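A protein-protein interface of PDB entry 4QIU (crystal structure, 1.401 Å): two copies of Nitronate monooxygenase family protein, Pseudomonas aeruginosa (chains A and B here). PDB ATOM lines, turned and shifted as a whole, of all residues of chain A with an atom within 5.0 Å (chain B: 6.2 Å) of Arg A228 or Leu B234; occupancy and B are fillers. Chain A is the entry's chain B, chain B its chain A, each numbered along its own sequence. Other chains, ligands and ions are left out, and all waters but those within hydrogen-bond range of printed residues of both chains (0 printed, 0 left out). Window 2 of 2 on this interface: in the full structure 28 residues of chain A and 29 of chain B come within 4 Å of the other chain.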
ATOM      1  N   ASP A 226      16.569 -18.036  12.499  1.00  0.00           N
ATOM      2  CA  ASP A 226      16.318 -17.334  13.746  1.00  0.00           C
ATOM      3  C   ASP A 226      15.779 -15.945  13.455  1.00  0.00           C
ATOM      4  O   ASP A 226      15.633 -15.561  12.295  1.00  0.00           O
ATOM      5  CB  ASP A 226      17.589 -17.271  14.606  1.00  0.00           C
ATOM      6  CG  ASP A 226      18.797 -16.742  13.851  1.00  0.00           C
ATOM      7  OD1 ASP A 226      18.628 -15.944  12.909  1.00  0.00           O
ATOM      8  OD2 ASP A 226      19.930 -17.120  14.218  1.00  0.00           O
ATOM      9  N   GLY A 227      15.456 -15.200  14.507  1.00  0.00           N
ATOM     10  CA  GLY A 227      14.868 -13.886  14.341  1.00  0.00           C
ATOM     11  C   GLY A 227      15.799 -12.899  13.668  1.00  0.00           C
ATOM     12  O   GLY A 227      15.328 -12.004  12.976  1.00  0.00           O
ATOM     13  N   ARG A 228      17.102 -13.041  13.893  1.00  0.00           N
ATOM     14  CA  ARG A 228      18.077 -12.193  13.213  1.00  0.00           C
ATOM     15  C   ARG A 228      17.960 -12.385  11.695  1.00  0.00           C
ATOM     16  O   ARG A 228      17.996 -11.422  10.936  1.00  0.00           O
ATOM     17  CB  ARG A 228      19.491 -12.501  13.695  1.00  0.00           C
ATOM     18  CG  ARG A 228      19.852 -11.851  15.025  1.00  0.00           C
ATOM     19  CD  ARG A 228      21.306 -12.113  15.372  1.00  0.00           C
ATOM     20  NE  ARG A 228      21.722 -11.386  16.571  1.00  0.00           N
ATOM     21  CZ  ARG A 228      22.296 -10.186  16.564  1.00  0.00           C
ATOM     22  NH1 ARG A 228      22.540  -9.561  15.415  1.00  0.00           N
ATOM     23  NH2 ARG A 228      22.633  -9.611  17.711  1.00  0.00           N
ATOM     24  N   GLY A 229      17.804 -13.634  11.267  1.00  0.00           N
ATOM     25  CA  GLY A 229      17.604 -13.944   9.857  1.00  0.00           C
ATOM     26  C   GLY A 229      16.327 -13.341   9.309  1.00  0.00           C
ATOM     27  O   GLY A 229      16.307 -12.802   8.198  1.00  0.00           O
ATOM     28  N   ILE A 230      15.253 -13.418  10.090  1.00  0.00           N
ATOM     29  CA  ILE A 230      13.976 -12.860   9.686  1.00  0.00           C
ATOM     30  C   ILE A 230      14.105 -11.338   9.569  1.00  0.00           C
ATOM     31  O   ILE A 230      13.673 -10.739   8.575  1.00  0.00           O
ATOM     32  CB  ILE A 230      12.854 -13.231  10.683  1.00  0.00           C
ATOM     33  CG1 ILE A 230      12.683 -14.748  10.754  1.00  0.00           C
ATOM     34  CG2 ILE A 230      11.549 -12.595  10.255  1.00  0.00           C
ATOM     35  CD1 ILE A 230      11.662 -15.168  11.795  1.00  0.00           C
ATOM     36  N   ARG A 231      14.722 -10.719  10.572  1.00  0.00           N
ATOM     37  CA  ARG A 231      14.968  -9.276  10.534  1.00  0.00           C
ATOM     38  C   ARG A 231      15.811  -8.865   9.328  1.00  0.00           C
ATOM     39  O   ARG A 231      15.535  -7.847   8.690  1.00  0.00           O
ATOM     40  CB  ARG A 231      15.644  -8.811  11.822  1.00  0.00           C
ATOM     41  CG  ARG A 231      14.717  -8.836  13.026  1.00  0.00           C
ATOM     42  CD  ARG A 231      15.483  -8.563  14.317  1.00  0.00           C
ATOM     43  NE  ARG A 231      14.694  -7.756  15.240  1.00  0.00           N
ATOM     44  CZ  ARG A 231      14.848  -6.449  15.425  1.00  0.00           C
ATOM     45  NH1 ARG A 231      15.788  -5.777  14.773  1.00  0.00           N
ATOM     46  NH2 ARG A 231      14.070  -5.816  16.283  1.00  0.00           N
ATOM     47  N   ALA A 232      16.831  -9.660   9.016  1.00  0.00           N
ATOM     48  CA  ALA A 232      17.663  -9.422   7.835  1.00  0.00           C
ATOM     49  C   ALA A 232      16.828  -9.450   6.553  1.00  0.00           C
ATOM     50  O   ALA A 232      16.960  -8.566   5.694  1.00  0.00           O
ATOM     51  CB  ALA A 232      18.778 -10.452   7.771  1.00  0.00           C
ATOM     52  N   GLU A 353      12.625 -13.284  19.007  1.00  0.00           N
ATOM     53  CA  GLU A 353      13.884 -12.895  18.374  1.00  0.00           C
ATOM     54  C   GLU A 353      13.658 -11.811  17.318  1.00  0.00           C
ATOM     55  O   GLU A 353      14.483 -10.913  17.156  1.00  0.00           O
ATOM     56  CB  GLU A 353      14.563 -14.121  17.753  1.00  0.00           C
ATOM     57  CG  GLU A 353      15.006 -15.145  18.783  1.00  0.00           C
ATOM     58  CD  GLU A 353      15.501 -16.444  18.182  1.00  0.00           C
ATOM     59  OE1 GLU A 353      15.264 -16.705  16.980  1.00  0.00           O
ATOM     60  OE2 GLU A 353      16.120 -17.223  18.928  1.00  0.00           O
ATOM     61  N   THR B   7      29.201  -2.293  14.910  1.00  0.00           N
ATOM     62  CA  THR B   7      29.867  -1.364  13.995  1.00  0.00           C
ATOM     63  C   THR B   7      30.692  -0.345  14.764  1.00  0.00           C
ATOM     64  O   THR B   7      31.704   0.136  14.257  1.00  0.00           O
ATOM     65  CB  THR B   7      28.874  -0.640  13.074  1.00  0.00           C
ATOM     66  OG1 THR B   7      27.877   0.019  13.856  1.00  0.00           O
ATOM     67  CG2 THR B   7      28.203  -1.638  12.143  1.00  0.00           C
ATOM     68  N   PRO B  19      31.241   1.780   8.790  1.00  0.00           N
ATOM     69  CA  PRO B  19      31.595   0.350   8.688  1.00  0.00           C
ATOM     70  C   PRO B  19      31.455  -0.209   7.270  1.00  0.00           C
ATOM     71  O   PRO B  19      30.775  -1.228   7.067  1.00  0.00           O
ATOM     72  CB  PRO B  19      30.581  -0.320   9.623  1.00  0.00           C
ATOM     73  CG  PRO B  19      29.367   0.532   9.476  1.00  0.00           C
ATOM     74  CD  PRO B  19      29.871   1.965   9.305  1.00  0.00           C
ATOM     75  N   ARG B 208      25.756 -15.239   9.089  1.00  0.00           N
ATOM     76  CA  ARG B 208      25.105 -15.670  10.323  1.00  0.00           C
ATOM     77  C   ARG B 208      25.929 -16.753  11.022  1.00  0.00           C
ATOM     78  O   ARG B 208      26.100 -16.726  12.236  1.00  0.00           O
ATOM     79  CB  ARG B 208      23.698 -16.184  10.045  1.00  0.00           C
ATOM     80  CG  ARG B 208      22.900 -16.471  11.313  1.00  0.00           C
ATOM     81  CD  ARG B 208      22.335 -15.194  11.943  1.00  0.00           C
ATOM     82  NE  ARG B 208      21.963 -15.440  13.331  1.00  0.00           N
ATOM     83  CZ  ARG B 208      22.682 -15.047  14.377  1.00  0.00           C
ATOM     84  NH1 ARG B 208      22.269 -15.339  15.605  1.00  0.00           N
ATOM     85  NH2 ARG B 208      23.806 -14.350  14.205  1.00  0.00           N
ATOM     86  N   GLY B 229      20.894  -3.639   2.203  1.00  0.00           N
ATOM     87  CA  GLY B 229      21.795  -4.786   2.278  1.00  0.00           C
ATOM     88  C   GLY B 229      22.777  -4.687   3.434  1.00  0.00           C
ATOM     89  O   GLY B 229      23.062  -5.682   4.101  1.00  0.00           O
ATOM     90  N   ILE B 230      23.275  -3.480   3.696  1.00  0.00           N
ATOM     91  CA  ILE B 230      24.136  -3.276   4.859  1.00  0.00           C
ATOM     92  C   ILE B 230      23.369  -3.552   6.157  1.00  0.00           C
ATOM     93  O   ILE B 230      23.868  -4.254   7.042  1.00  0.00           O
ATOM     94  CB  ILE B 230      24.716  -1.854   4.883  1.00  0.00           C
ATOM     95  CG1 ILE B 230      25.449  -1.579   3.565  1.00  0.00           C
ATOM     96  CG2 ILE B 230      25.634  -1.696   6.088  1.00  0.00           C
ATOM     97  CD1 ILE B 230      26.083  -0.185   3.480  1.00  0.00           C
ATOM     98  N   ARG B 231      22.158  -3.008   6.271  1.00  0.00           N
ATOM     99  CA  ARG B 231      21.335  -3.238   7.447  1.00  0.00           C
ATOM    100  C   ARG B 231      21.052  -4.723   7.641  1.00  0.00           C
ATOM    101  O   ARG B 231      21.113  -5.222   8.762  1.00  0.00           O
ATOM    102  CB  ARG B 231      20.033  -2.441   7.348  1.00  0.00           C
ATOM    103  CG  ARG B 231      20.263  -0.924   7.516  1.00  0.00           C
ATOM    104  CD  ARG B 231      19.020  -0.107   7.171  1.00  0.00           C
ATOM    105  NE  ARG B 231      17.900  -0.400   8.061  1.00  0.00           N
ATOM    106  CZ  ARG B 231      17.686   0.226   9.216  1.00  0.00           C
ATOM    107  NH1 ARG B 231      18.506   1.192   9.612  1.00  0.00           N
ATOM    108  NH2 ARG B 231      16.642  -0.101   9.965  1.00  0.00           N
ATOM    109  N   ALA B 232      20.784  -5.434   6.547  1.00  0.00           N
ATOM    110  CA  ALA B 232      20.545  -6.873   6.631  1.00  0.00           C
ATOM    111  C   ALA B 232      21.781  -7.606   7.145  1.00  0.00           C
ATOM    112  O   ALA B 232      21.674  -8.491   7.998  1.00  0.00           O
ATOM    113  CB  ALA B 232      20.116  -7.434   5.264  1.00  0.00           C
ATOM    114  N   ALA B 233      22.958  -7.236   6.642  1.00  0.00           N
ATOM    115  CA  ALA B 233      24.205  -7.842   7.096  1.00  0.00           C
ATOM    116  C   ALA B 233      24.414  -7.599   8.576  1.00  0.00           C
ATOM    117  O   ALA B 233      24.866  -8.493   9.300  1.00  0.00           O
ATOM    118  CB  ALA B 233      25.396  -7.308   6.309  1.00  0.00           C
ATOM    119  N   LEU B 234      24.081  -6.393   9.029  1.00  0.00           N
ATOM    120  CA  LEU B 234      24.232  -6.080  10.443  1.00  0.00           C
ATOM    121  C   LEU B 234      23.259  -6.900  11.290  1.00  0.00           C
ATOM    122  O   LEU B 234      23.620  -7.365  12.370  1.00  0.00           O
ATOM    123  CB  LEU B 234      24.036  -4.578  10.682  1.00  0.00           C
ATOM    124  CG  LEU B 234      25.098  -3.720   9.977  1.00  0.00           C
ATOM    125  CD1 LEU B 234      24.906  -2.247  10.287  1.00  0.00           C
ATOM    126  CD2 LEU B 234      26.524  -4.175  10.323  1.00  0.00           C
ATOM    127  N   GLU B 235      22.030  -7.082  10.816  1.00  0.00           N
ATOM    128  CA  GLU B 235      21.079  -7.912  11.547  1.00  0.00           C
ATOM    129  C   GLU B 235      21.603  -9.335  11.715  1.00  0.00           C
ATOM    130  O   GLU B 235      21.374  -9.976  12.738  1.00  0.00           O
ATOM    131  CB  GLU B 235      19.713  -7.932  10.848  1.00  0.00           C
ATOM    132  CG  GLU B 235      18.907  -6.647  11.001  1.00  0.00           C
ATOM    133  CD  GLU B 235      18.421  -6.390  12.423  1.00  0.00           C
ATOM    134  OE1 GLU B 235      18.483  -7.309  13.266  1.00  0.00           O
ATOM    135  OE2 GLU B 235      17.962  -5.259  12.684  1.00  0.00           O
ATOM    136  N   LEU B 236      22.327  -9.825  10.715  1.00  0.00           N
ATOM    137  CA  LEU B 236      22.869 -11.181  10.764  1.00  0.00           C
ATOM    138  C   LEU B 236      24.036 -11.308  11.730  1.00  0.00           C
ATOM    139  O   LEU B 236      24.464 -12.416  12.064  1.00  0.00           O
ATOM    140  CB  LEU B 236      23.314 -11.610   9.368  1.00  0.00           C
ATOM    141  CG  LEU B 236      22.170 -11.727   8.372  1.00  0.00           C
ATOM    142  CD1 LEU B 236      22.755 -11.942   6.977  1.00  0.00           C
ATOM    143  CD2 LEU B 236      21.237 -12.885   8.742  1.00  0.00           C
ATOM    144  N   GLY B 237      24.570 -10.165  12.152  1.00  0.00           N
ATOM    145  CA  GLY B 237      25.646 -10.148  13.129  1.00  0.00           C
ATOM    146  C   GLY B 237      26.972  -9.624  12.617  1.00  0.00           C
ATOM    147  O   GLY B 237      27.964  -9.664  13.329  1.00  0.00           O
ATOM    148  N   ALA B 238      27.012  -9.142  11.380  1.00  0.00           N
ATOM    149  CA  ALA B 238      28.246  -8.567  10.848  1.00  0.00           C
ATOM    150  C   ALA B 238      28.629  -7.282  11.582  1.00  0.00           C
ATOM    151  O   ALA B 238      27.773  -6.602  12.146  1.00  0.00           O
ATOM    152  CB  ALA B 238      28.107  -8.287   9.356  1.00  0.00           C
ATOM    153  N   SER B 239      29.922  -6.968  11.559  1.00  0.00           N
ATOM    154  CA  SER B 239      30.457  -5.742  12.152  1.00  0.00           C
ATOM    155  C   SER B 239      30.691  -4.667  11.093  1.00  0.00           C
ATOM    156  O   SER B 239      30.886  -3.492  11.420  1.00  0.00           O
ATOM    157  CB  SER B 239      31.770  -6.024  12.886  1.00  0.00           C
ATOM    158  OG  SER B 239      31.580  -6.910  13.978  1.00  0.00           O
ATOM    159  N   ALA B 240      30.685  -5.078   9.828  1.00  0.00           N
ATOM    160  CA  ALA B 240      30.948  -4.176   8.710  1.00  0.00           C
ATOM    161  C   ALA B 240      30.582  -4.885   7.413  1.00  0.00           C
ATOM    162  O   ALA B 240      30.229  -6.065   7.437  1.00  0.00           O
ATOM    163  CB  ALA B 240      32.418  -3.735   8.687  1.00  0.00           C
ATOM    164  N   VAL B 241      30.671  -4.164   6.296  1.00  0.00           N
ATOM    165  CA  VAL B 241      30.492  -4.764   4.976  1.00  0.00           C
ATOM    166  C   VAL B 241      31.672  -4.442   4.073  1.00  0.00           C
ATOM    167  O   VAL B 241      32.379  -3.440   4.274  1.00  0.00           O
ATOM    168  CB  VAL B 241      29.195  -4.279   4.293  1.00  0.00           C
ATOM    169  CG1 VAL B 241      27.977  -4.664   5.129  1.00  0.00           C
ATOM    170  CG2 VAL B 241      29.229  -2.764   4.023  1.00  0.00           C
ATOM    171  N   LEU B 354      21.754   3.383   5.160  1.00  0.00           N
ATOM    172  CA  LEU B 354      22.001   2.592   6.368  1.00  0.00           C
ATOM    173  C   LEU B 354      21.263   3.154   7.591  1.00  0.00           C
ATOM    174  O   LEU B 354      20.763   2.406   8.437  1.00  0.00           O
ATOM    175  CB  LEU B 354      23.506   2.532   6.643  1.00  0.00           C
ATOM    176  CG  LEU B 354      24.011   2.004   7.990  1.00  0.00           C
ATOM    177  CD1 LEU B 354      23.546   0.574   8.242  1.00  0.00           C
ATOM    178  CD2 LEU B 354      25.528   2.087   8.049  1.00  0.00           C
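OD2 of Asp A226 lies within salt-bridge range of NE of Arg B208, 2.8 Å away. NH1 of Arg A228 is in hydrogen-bond range of O of Glu B235, at 2.9 Å. The guanidinium group of Arg A231 lies within salt-bridge range of the side-chain carboxylate of Glu B235, at 3.1 Å.
The guanidinium group (NH2) of Arg B208 lies within hydrogen-bond range of the backbone carbonyl oxygen (O) of Leu B236 (3.0 Å). N of Arg A228 sits close to OD1 of Asp A226. OD1 of Asp A226 lies within hydrogen-bond range of N of Gly A229, at 3.0 Å.
Among the printed residues, merely in contact across the chains: Arg A228 with Arg B208 (3.4 Å), Arg A228 with Leu B234 (3.9 Å), Arg A228 with Gly B237 (3.9 Å), Gly A229 with Leu B236 (3.9 Å), Ala A232 with Ala B232 (3.4 Å), Ala A232 with Glu B235 (3.8 Å) and Ala A232 with Leu B236 (3.6 Å).
Arg A228 touches four residues of chain B. Of the printed residues of chain B, Gly A229 touches Leu B236. Thr B7 touches none of the printed residues of chain A. Of the printed residues of chain A, Arg B208 touches Asp A226 and Arg A228. Of the printed residues of chain A, Ala B232 touches Ala A232. Of chain A, only Arg A228 comes within 4 Å of Leu B234. Of the printed residues of chain A, Glu B235 touches Arg A228 (2.9 Å), Arg A231 (3.1 Å) and Ala A232 (3.8 Å). Printed residues of chain A within 4 Å of Gly B237: Arg A228. The nearest residue of chain B that does not touch Arg A228 is Leu B236 (4.2 Å). The nearest printed residue of chain A that does not touch Leu B234 is Ala A232 (6.7 Å).
Of the 17 printed residues of chain B, 6 touch a printed residue of chain A. Hydrophobic or aromatic side chains of chain B within 4 Å of the printed part of chain A: Ala B232 and Leu B236. Of the 8 printed residues of chain A, 5 touch a printed residue of chain B. Printed residues of chain A that touch a printed residue of chain B: Asp A226, Arg A228, Gly A229, Arg A231 and Ala A232. Among the printed residues, 10 pairs touch across the chains.
Ala A232 touches its own counterpart, Ala B232.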
